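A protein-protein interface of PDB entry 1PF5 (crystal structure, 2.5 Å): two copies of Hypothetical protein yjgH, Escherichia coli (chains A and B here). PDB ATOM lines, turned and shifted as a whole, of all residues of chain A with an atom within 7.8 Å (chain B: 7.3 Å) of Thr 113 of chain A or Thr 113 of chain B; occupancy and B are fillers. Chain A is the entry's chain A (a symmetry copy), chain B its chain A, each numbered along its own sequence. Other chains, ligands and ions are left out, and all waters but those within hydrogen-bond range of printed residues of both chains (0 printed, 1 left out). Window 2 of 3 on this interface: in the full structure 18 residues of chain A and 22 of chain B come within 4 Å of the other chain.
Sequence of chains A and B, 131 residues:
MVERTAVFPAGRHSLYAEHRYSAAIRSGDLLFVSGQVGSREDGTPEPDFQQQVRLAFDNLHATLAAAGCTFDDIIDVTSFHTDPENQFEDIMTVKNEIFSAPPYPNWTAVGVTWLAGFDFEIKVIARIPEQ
Printed residues of chain A within 4 Å of Thr 113 of chain B: Thr 113 (3.5 Å). Printed residues of chain B within 4 Å of Trp 114 of chain A: Pro 84 (3.2 Å), Glu 85 (3.6 Å) and Gly 111 (3.1 Å). Of the printed residues of chain A, Val 110 of chain B touches Phe 80 (3.9 Å) and Val 112 (3.1 Å). Of the printed residues of chain A, Val 112 of chain B touches Thr 113 (3.9 Å). His 81 of chain A touches none of the printed residues of chain B. The nearest printed residue of chain B that does not touch Thr 113 of chain A is His 81 of chain B (4.9 Å). The nearest residue of chain A that does not touch Thr 113 of chain B is Gly 111 of chain A (5.8 Å).
O of Gly 111 of chain B sits at hydrogen-bond distance from N of Thr 113 of chain A (2.9 Å). O of Trp 114 of chain A sits at hydrogen-bond distance from N of Gly 111 of chain B (3.1 Å).
The backbone carbonyl oxygen (O) of His 81 of chain A lies within hydrogen-bond range of the backbone NH (N) of Val 112 of chain A (2.8 Å). The backbone NH (N) of Val 112 of chain B lies within hydrogen-bond range of the backbone carbonyl oxygen (O) of His 81 of chain B, at 2.8 Å. N of His 81 of chain B sits at hydrogen-bond distance from O of Val 110 of chain B (2.9 Å).
CD1 of Phe 80 of chain A touches CG2 of Val 110 of chain B, 3.9 Å away. CG1 of Val 112 of chain A touches CG1 of Val 110 of chain B (3.1 Å). CB of Val 112 of chain A touches O of Gly 111 of chain B, 3.3 Å away. OG1 of Thr 113 of chain A touches N of Val 112 of chain B, at 3.9 Å. CG2 of Thr 113 of chain A touches CG2 of Thr 113 of chain B (3.5 Å). Trp 114 of chain A touches Pro 84 of chain B. NE1 of Trp 114 of chain A touches OE1 of Glu 85 of chain B (3.6 Å).
Val 112 of chain A touches Gly 111 of chain B, but with the chains exchanged Gly 111 of chain A does not touch Val 112 of chain B (6.3 Å). Thr 113 of chain A touches Gly 111 of chain B, but with the chains exchanged Gly 111 of chain A does not touch Thr 113 of chain B (5.8 Å). Thr 113 of chain A touches its own counterpart, Thr 113 of chain B. Trp 114 of chain A touches Gly 111 of chain B, but with the chains exchanged Gly 111 of chain A does not touch Trp 114 of chain B (8.9 Å). Positions printed for both chains: 81, 82, 83, 110, 111, 112, 113, 114, 115, 116 and 118. Of the 9 pairs that touch across the chains among the printed residues, 1 has its exchanged pair printed and touching as well.
Of the 13 printed residues of chain A, 4 touch a printed residue of chain B. Hydrophobic or aromatic side chains of chain A that line the printed part of chain B: Phe 80, Val 112 and Trp 114. Of the 13 printed residues of chain B, 6 touch a printed residue of chain A. Printed residues of chain B that touch a printed residue of chain A: Pro 84, Glu 85, Val 110, Gly 111, Val 112 and Thr 113. Among the printed residues, 9 pairs touch across the chains. Among the printed residues, no Asp or Glu carboxylate lies within 4 Å of a Lys or Arg side-chain nitrogen of the other chain.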
ATOM      1  N   PHE A  80       5.657  -2.106   3.819  1.00  0.00           N
ATOM      2  CA  PHE A  80       6.520  -3.275   3.941  1.00  0.00           C
ATOM      3  C   PHE A  80       5.723  -4.409   4.565  1.00  0.00           C
ATOM      4  O   PHE A  80       4.902  -4.190   5.459  1.00  0.00           O
ATOM      5  CB  PHE A  80       7.720  -2.921   4.807  1.00  0.00           C
ATOM      6  CG  PHE A  80       8.421  -1.681   4.360  1.00  0.00           C
ATOM      7  CD1 PHE A  80       9.322  -1.723   3.302  1.00  0.00           C
ATOM      8  CD2 PHE A  80       8.129  -0.456   4.953  1.00  0.00           C
ATOM      9  CE1 PHE A  80       9.923  -0.562   2.834  1.00  0.00           C
ATOM     10  CE2 PHE A  80       8.721   0.716   4.497  1.00  0.00           C
ATOM     11  CZ  PHE A  80       9.623   0.665   3.432  1.00  0.00           C
ATOM     12  N   HIS A  81       5.986  -5.625   4.106  1.00  0.00           N
ATOM     13  CA  HIS A  81       5.250  -6.784   4.575  1.00  0.00           C
ATOM     14  C   HIS A  81       6.154  -7.971   4.845  1.00  0.00           C
ATOM     15  O   HIS A  81       7.030  -8.288   4.043  1.00  0.00           O
ATOM     16  CB  HIS A  81       4.208  -7.129   3.518  1.00  0.00           C
ATOM     17  CG  HIS A  81       3.486  -5.926   2.998  1.00  0.00           C
ATOM     18  ND1 HIS A  81       2.547  -5.246   3.744  1.00  0.00           N
ATOM     19  CD2 HIS A  81       3.655  -5.209   1.862  1.00  0.00           C
ATOM     20  CE1 HIS A  81       2.172  -4.160   3.091  1.00  0.00           C
ATOM     21  NE2 HIS A  81       2.832  -4.113   1.947  1.00  0.00           N
ATOM     22  N   THR A  82       5.928  -8.627   5.978  1.00  0.00           N
ATOM     23  CA  THR A  82       6.722  -9.779   6.374  1.00  0.00           C
ATOM     24  C   THR A  82       6.279 -11.056   5.668  1.00  0.00           C
ATOM     25  O   THR A  82       7.035 -12.021   5.579  1.00  0.00           O
ATOM     26  CB  THR A  82       6.633  -9.996   7.875  1.00  0.00           C
ATOM     27  OG1 THR A  82       5.255 -10.104   8.246  1.00  0.00           O
ATOM     28  CG2 THR A  82       7.275  -8.829   8.625  1.00  0.00           C
ATOM     29  N   ASP A  83       5.051 -11.060   5.166  1.00  0.00           N
ATOM     30  CA  ASP A  83       4.522 -12.215   4.452  1.00  0.00           C
ATOM     31  C   ASP A  83       3.341 -11.725   3.629  1.00  0.00           C
ATOM     32  O   ASP A  83       2.203 -12.153   3.823  1.00  0.00           O
ATOM     33  CB  ASP A  83       4.085 -13.294   5.444  1.00  0.00           C
ATOM     34  CG  ASP A  83       3.415 -14.485   4.767  1.00  0.00           C
ATOM     35  OD1 ASP A  83       3.705 -14.754   3.577  1.00  0.00           O
ATOM     36  OD2 ASP A  83       2.603 -15.159   5.441  1.00  0.00           O
ATOM     37  N   VAL A 110       6.248  -3.681  -0.712  1.00  0.00           N
ATOM     38  CA  VAL A 110       7.400  -4.560  -0.831  1.00  0.00           C
ATOM     39  C   VAL A 110       7.481  -5.604   0.275  1.00  0.00           C
ATOM     40  O   VAL A 110       7.111  -5.336   1.420  1.00  0.00           O
ATOM     41  CB  VAL A 110       8.697  -3.724  -0.811  1.00  0.00           C
ATOM     42  CG1 VAL A 110       9.884  -4.614  -0.760  1.00  0.00           C
ATOM     43  CG2 VAL A 110       8.764  -2.855  -2.042  1.00  0.00           C
ATOM     44  N   GLY A 111       7.981  -6.787  -0.077  1.00  0.00           N
ATOM     45  CA  GLY A 111       8.129  -7.856   0.894  1.00  0.00           C
ATOM     46  C   GLY A 111       9.480  -7.783   1.580  1.00  0.00           C
ATOM     47  O   GLY A 111      10.524  -7.815   0.923  1.00  0.00           O
ATOM     48  N   VAL A 112       9.470  -7.674   2.903  1.00  0.00           N
ATOM     49  CA  VAL A 112      10.708  -7.598   3.659  1.00  0.00           C
ATOM     50  C   VAL A 112      10.847  -8.785   4.600  1.00  0.00           C
ATOM     51  O   VAL A 112       9.902  -9.546   4.802  1.00  0.00           O
ATOM     52  CB  VAL A 112      10.785  -6.299   4.463  1.00  0.00           C
ATOM     53  CG1 VAL A 112      10.579  -5.129   3.534  1.00  0.00           C
ATOM     54  CG2 VAL A 112       9.744  -6.302   5.570  1.00  0.00           C
ATOM     55  N   THR A 113      12.032  -8.934   5.179  1.00  0.00           N
ATOM     56  CA  THR A 113      12.317 -10.053   6.066  1.00  0.00           C
ATOM     57  C   THR A 113      12.153  -9.757   7.548  1.00  0.00           C
ATOM     58  O   THR A 113      12.085 -10.678   8.357  1.00  0.00           O
ATOM     59  CB  THR A 113      13.763 -10.555   5.866  1.00  0.00           C
ATOM     60  OG1 THR A 113      14.679  -9.671   6.523  1.00  0.00           O
ATOM     61  CG2 THR A 113      14.105 -10.602   4.396  1.00  0.00           C
ATOM     62  N   TRP A 114      12.078  -8.482   7.907  1.00  0.00           N
ATOM     63  CA  TRP A 114      11.993  -8.106   9.310  1.00  0.00           C
ATOM     64  C   TRP A 114      11.422  -6.692   9.487  1.00  0.00           C
ATOM     65  O   TRP A 114      11.665  -5.809   8.665  1.00  0.00           O
ATOM     66  CB  TRP A 114      13.411  -8.198   9.887  1.00  0.00           C
ATOM     67  CG  TRP A 114      13.614  -7.738  11.291  1.00  0.00           C
ATOM     68  CD1 TRP A 114      13.577  -8.501  12.423  1.00  0.00           C
ATOM     69  CD2 TRP A 114      13.949  -6.413  11.709  1.00  0.00           C
ATOM     70  NE1 TRP A 114      13.876  -7.731  13.524  1.00  0.00           N
ATOM     71  CE2 TRP A 114      14.107  -6.444  13.113  1.00  0.00           C
ATOM     72  CE3 TRP A 114      14.133  -5.199  11.033  1.00  0.00           C
ATOM     73  CZ2 TRP A 114      14.442  -5.307  13.856  1.00  0.00           C
ATOM     74  CZ3 TRP A 114      14.466  -4.067  11.770  1.00  0.00           C
ATOM     75  CH2 TRP A 114      14.616  -4.131  13.171  1.00  0.00           C
ATOM     76  N   LEU A 115      10.648  -6.497  10.551  1.00  0.00           N
ATOM     77  CA  LEU A 115      10.064  -5.199  10.864  1.00  0.00           C
ATOM     78  C   LEU A 115       9.970  -5.060  12.387  1.00  0.00           C
ATOM     79  O   LEU A 115       8.943  -4.656  12.940  1.00  0.00           O
ATOM     80  CB  LEU A 115       8.679  -5.042  10.217  1.00  0.00           C
ATOM     81  CG  LEU A 115       8.575  -4.965   8.682  1.00  0.00           C
ATOM     82  CD1 LEU A 115       7.109  -4.834   8.298  1.00  0.00           C
ATOM     83  CD2 LEU A 115       9.371  -3.788   8.128  1.00  0.00           C
ATOM     84  N   ALA A 116      11.064  -5.418  13.054  1.00  0.00           N
ATOM     85  CA  ALA A 116      11.186  -5.331  14.503  1.00  0.00           C
ATOM     86  C   ALA A 116      10.053  -5.983  15.281  1.00  0.00           C
ATOM     87  O   ALA A 116       9.633  -5.466  16.316  1.00  0.00           O
ATOM     88  CB  ALA A 116      11.316  -3.879  14.911  1.00  0.00           C
ATOM     89  N   GLY A 117       9.565  -7.116  14.793  1.00  0.00           N
ATOM     90  CA  GLY A 117       8.489  -7.798  15.483  1.00  0.00           C
ATOM     91  C   GLY A 117       7.120  -7.581  14.869  1.00  0.00           C
ATOM     92  O   GLY A 117       6.181  -8.332  15.144  1.00  0.00           O
ATOM     93  N   PHE A 118       6.995  -6.558  14.031  1.00  0.00           N
ATOM     94  CA  PHE A 118       5.718  -6.274  13.391  1.00  0.00           C
ATOM     95  C   PHE A 118       5.606  -6.969  12.044  1.00  0.00           C
ATOM     96  O   PHE A 118       6.594  -7.474  11.509  1.00  0.00           O
ATOM     97  CB  PHE A 118       5.540  -4.764  13.246  1.00  0.00           C
ATOM     98  CG  PHE A 118       5.591  -4.033  14.560  1.00  0.00           C
ATOM     99  CD1 PHE A 118       6.812  -3.641  15.105  1.00  0.00           C
ATOM    100  CD2 PHE A 118       4.423  -3.811  15.293  1.00  0.00           C
ATOM    101  CE1 PHE A 118       6.870  -3.042  16.369  1.00  0.00           C
ATOM    102  CE2 PHE A 118       4.465  -3.216  16.552  1.00  0.00           C
ATOM    103  CZ  PHE A 118       5.693  -2.832  17.094  1.00  0.00           C
ATOM    104  N   HIS B  81      18.782  -3.703   6.464  1.00  0.00           N
ATOM    105  CA  HIS B  81      19.618  -4.627   7.206  1.00  0.00           C
ATOM    106  C   HIS B  81      19.499  -6.050   6.695  1.00  0.00           C
ATOM    107  O   HIS B  81      18.397  -6.538   6.447  1.00  0.00           O
ATOM    108  CB  HIS B  81      19.211  -4.545   8.672  1.00  0.00           C
ATOM    109  CG  HIS B  81      19.024  -3.139   9.146  1.00  0.00           C
ATOM    110  ND1 HIS B  81      20.082  -2.283   9.362  1.00  0.00           N
ATOM    111  CD2 HIS B  81      17.902  -2.402   9.323  1.00  0.00           C
ATOM    112  CE1 HIS B  81      19.620  -1.078   9.647  1.00  0.00           C
ATOM    113  NE2 HIS B  81      18.300  -1.123   9.628  1.00  0.00           N
ATOM    114  N   THR B  82      20.641  -6.712   6.547  1.00  0.00           N
ATOM    115  CA  THR B  82      20.682  -8.080   6.057  1.00  0.00           C
ATOM    116  C   THR B  82      20.356  -9.095   7.147  1.00  0.00           C
ATOM    117  O   THR B  82      19.979 -10.229   6.860  1.00  0.00           O
ATOM    118  CB  THR B  82      22.053  -8.401   5.487  1.00  0.00           C
ATOM    119  OG1 THR B  82      23.044  -8.127   6.484  1.00  0.00           O
ATOM    120  CG2 THR B  82      22.331  -7.554   4.245  1.00  0.00           C
ATOM    121  N   ASP B  83      20.503  -8.686   8.401  1.00  0.00           N
ATOM    122  CA  ASP B  83      20.203  -9.557   9.529  1.00  0.00           C
ATOM    123  C   ASP B  83      20.014  -8.662  10.744  1.00  0.00           C
ATOM    124  O   ASP B  83      20.755  -8.748  11.723  1.00  0.00           O
ATOM    125  CB  ASP B  83      21.349 -10.545   9.752  1.00  0.00           C
ATOM    126  CG  ASP B  83      21.152 -11.413  10.990  1.00  0.00           C
ATOM    127  OD1 ASP B  83      19.987 -11.643  11.396  1.00  0.00           O
ATOM    128  OD2 ASP B  83      22.173 -11.874  11.549  1.00  0.00           O
ATOM    129  N   PRO B  84      18.992  -7.796  10.692  1.00  0.00           N
ATOM    130  CA  PRO B  84      18.648  -6.844  11.748  1.00  0.00           C
ATOM    131  C   PRO B  84      18.622  -7.400  13.162  1.00  0.00           C
ATOM    132  O   PRO B  84      18.972  -6.700  14.106  1.00  0.00           O
ATOM    133  CB  PRO B  84      17.294  -6.317  11.299  1.00  0.00           C
ATOM    134  CG  PRO B  84      16.732  -7.455  10.535  1.00  0.00           C
ATOM    135  CD  PRO B  84      17.895  -7.895   9.717  1.00  0.00           C
ATOM    136  N   GLU B  85      18.213  -8.653  13.313  1.00  0.00           N
ATOM    137  CA  GLU B  85      18.141  -9.271  14.636  1.00  0.00           C
ATOM    138  C   GLU B  85      19.463  -9.259  15.390  1.00  0.00           C
ATOM    139  O   GLU B  85      19.519  -8.870  16.560  1.00  0.00           O
ATOM    140  CB  GLU B  85      17.644 -10.712  14.519  1.00  0.00           C
ATOM    141  CG  GLU B  85      16.154 -10.820  14.295  1.00  0.00           C
ATOM    142  CD  GLU B  85      15.356 -10.424  15.528  1.00  0.00           C
ATOM    143  OE1 GLU B  85      15.654  -9.367  16.139  1.00  0.00           O
ATOM    144  OE2 GLU B  85      14.422 -11.177  15.882  1.00  0.00           O
ATOM    145  N   VAL B 110      14.311  -1.482   7.928  1.00  0.00           N
ATOM    146  CA  VAL B 110      13.713  -2.651   7.302  1.00  0.00           C
ATOM    147  C   VAL B 110      14.710  -3.770   7.032  1.00  0.00           C
ATOM    148  O   VAL B 110      15.873  -3.512   6.715  1.00  0.00           O
ATOM    149  CB  VAL B 110      13.058  -2.246   5.964  1.00  0.00           C
ATOM    150  CG1 VAL B 110      12.593  -3.450   5.232  1.00  0.00           C
ATOM    151  CG2 VAL B 110      11.892  -1.324   6.224  1.00  0.00           C
ATOM    152  N   GLY B 111      14.237  -5.009   7.147  1.00  0.00           N
ATOM    153  CA  GLY B 111      15.085  -6.161   6.894  1.00  0.00           C
ATOM    154  C   GLY B 111      15.037  -6.559   5.431  1.00  0.00           C
ATOM    155  O   GLY B 111      13.965  -6.839   4.888  1.00  0.00           O
ATOM    156  N   VAL B 112      16.195  -6.575   4.781  1.00  0.00           N
ATOM    157  CA  VAL B 112      16.261  -6.944   3.377  1.00  0.00           C
ATOM    158  C   VAL B 112      17.095  -8.201   3.181  1.00  0.00           C
ATOM    159  O   VAL B 112      17.771  -8.660   4.100  1.00  0.00           O
ATOM    160  CB  VAL B 112      16.846  -5.808   2.536  1.00  0.00           C
ATOM    161  CG1 VAL B 112      16.056  -4.549   2.787  1.00  0.00           C
ATOM    162  CG2 VAL B 112      18.314  -5.604   2.875  1.00  0.00           C
ATOM    163  N   THR B 113      17.046  -8.750   1.974  1.00  0.00           N
ATOM    164  CA  THR B 113      17.758  -9.981   1.662  1.00  0.00           C
ATOM    165  C   THR B 113      19.117  -9.790   1.007  1.00  0.00           C
ATOM    166  O   THR B 113      19.917 -10.720   0.962  1.00  0.00           O
ATOM    167  CB  THR B 113      16.925 -10.871   0.715  1.00  0.00           C
ATOM    168  OG1 THR B 113      17.007 -10.366  -0.623  1.00  0.00           O
ATOM    169  CG2 THR B 113      15.476 -10.880   1.141  1.00  0.00           C
ATOM    170  N   TRP B 114      19.386  -8.591   0.509  1.00  0.00           N
ATOM    171  CA  TRP B 114      20.632  -8.339  -0.199  1.00  0.00           C
ATOM    172  C   TRP B 114      20.970  -6.843  -0.243  1.00  0.00           C
ATOM    173  O   TRP B 114      20.078  -6.000  -0.326  1.00  0.00           O
ATOM    174  CB  TRP B 114      20.467  -8.904  -1.615  1.00  0.00           C
ATOM    175  CG  TRP B 114      21.571  -8.659  -2.587  1.00  0.00           C
ATOM    176  CD1 TRP B 114      22.629  -9.479  -2.858  1.00  0.00           C
ATOM    177  CD2 TRP B 114      21.694  -7.540  -3.467  1.00  0.00           C
ATOM    178  NE1 TRP B 114      23.403  -8.940  -3.861  1.00  0.00           N
ATOM    179  CE2 TRP B 114      22.851  -7.748  -4.252  1.00  0.00           C
ATOM    180  CE3 TRP B 114      20.936  -6.378  -3.672  1.00  0.00           C
ATOM    181  CZ2 TRP B 114      23.270  -6.838  -5.228  1.00  0.00           C
ATOM    182  CZ3 TRP B 114      21.351  -5.471  -4.642  1.00  0.00           C
ATOM    183  CH2 TRP B 114      22.511  -5.708  -5.408  1.00  0.00           C
ATOM    184  N   LEU B 115      22.259  -6.526  -0.167  1.00  0.00           N
ATOM    185  CA  LEU B 115      22.730  -5.148  -0.229  1.00  0.00           C
ATOM    186  C   LEU B 115      24.102  -5.131  -0.913  1.00  0.00           C
ATOM    187  O   LEU B 115      25.050  -4.493  -0.449  1.00  0.00           O
ATOM    188  CB  LEU B 115      22.814  -4.525   1.173  1.00  0.00           C
ATOM    189  CG  LEU B 115      21.514  -4.277   1.961  1.00  0.00           C
ATOM    190  CD1 LEU B 115      21.870  -3.679   3.314  1.00  0.00           C
ATOM    191  CD2 LEU B 115      20.574  -3.345   1.204  1.00  0.00           C
ATOM    192  N   ALA B 116      24.186  -5.859  -2.023  1.00  0.00           N
ATOM    193  CA  ALA B 116      25.392  -5.949  -2.835  1.00  0.00           C
ATOM    194  C   ALA B 116      26.656  -6.303  -2.066  1.00  0.00           C
ATOM    195  O   ALA B 116      27.732  -5.784  -2.367  1.00  0.00           O
ATOM    196  CB  ALA B 116      25.595  -4.647  -3.580  1.00  0.00           C
ATOM    197  N   PHE B 118      27.057  -5.820   1.227  1.00  0.00           N
ATOM    198  CA  PHE B 118      27.088  -5.109   2.498  1.00  0.00           C
ATOM    199  C   PHE B 118      26.005  -5.610   3.440  1.00  0.00           C
ATOM    200  O   PHE B 118      25.097  -6.334   3.031  1.00  0.00           O
ATOM    201  CB  PHE B 118      26.950  -3.608   2.251  1.00  0.00           C
ATOM    202  CG  PHE B 118      28.031  -3.052   1.364  1.00  0.00           C
ATOM    203  CD1 PHE B 118      27.901  -3.095  -0.022  1.00  0.00           C
ATOM    204  CD2 PHE B 118      29.217  -2.561   1.916  1.00  0.00           C
ATOM    205  CE1 PHE B 118      28.943  -2.662  -0.851  1.00  0.00           C
ATOM    206  CE2 PHE B 118      30.263  -2.127   1.104  1.00  0.00           C
ATOM    207  CZ  PHE B 118      30.127  -2.179  -0.285  1.00  0.00           C
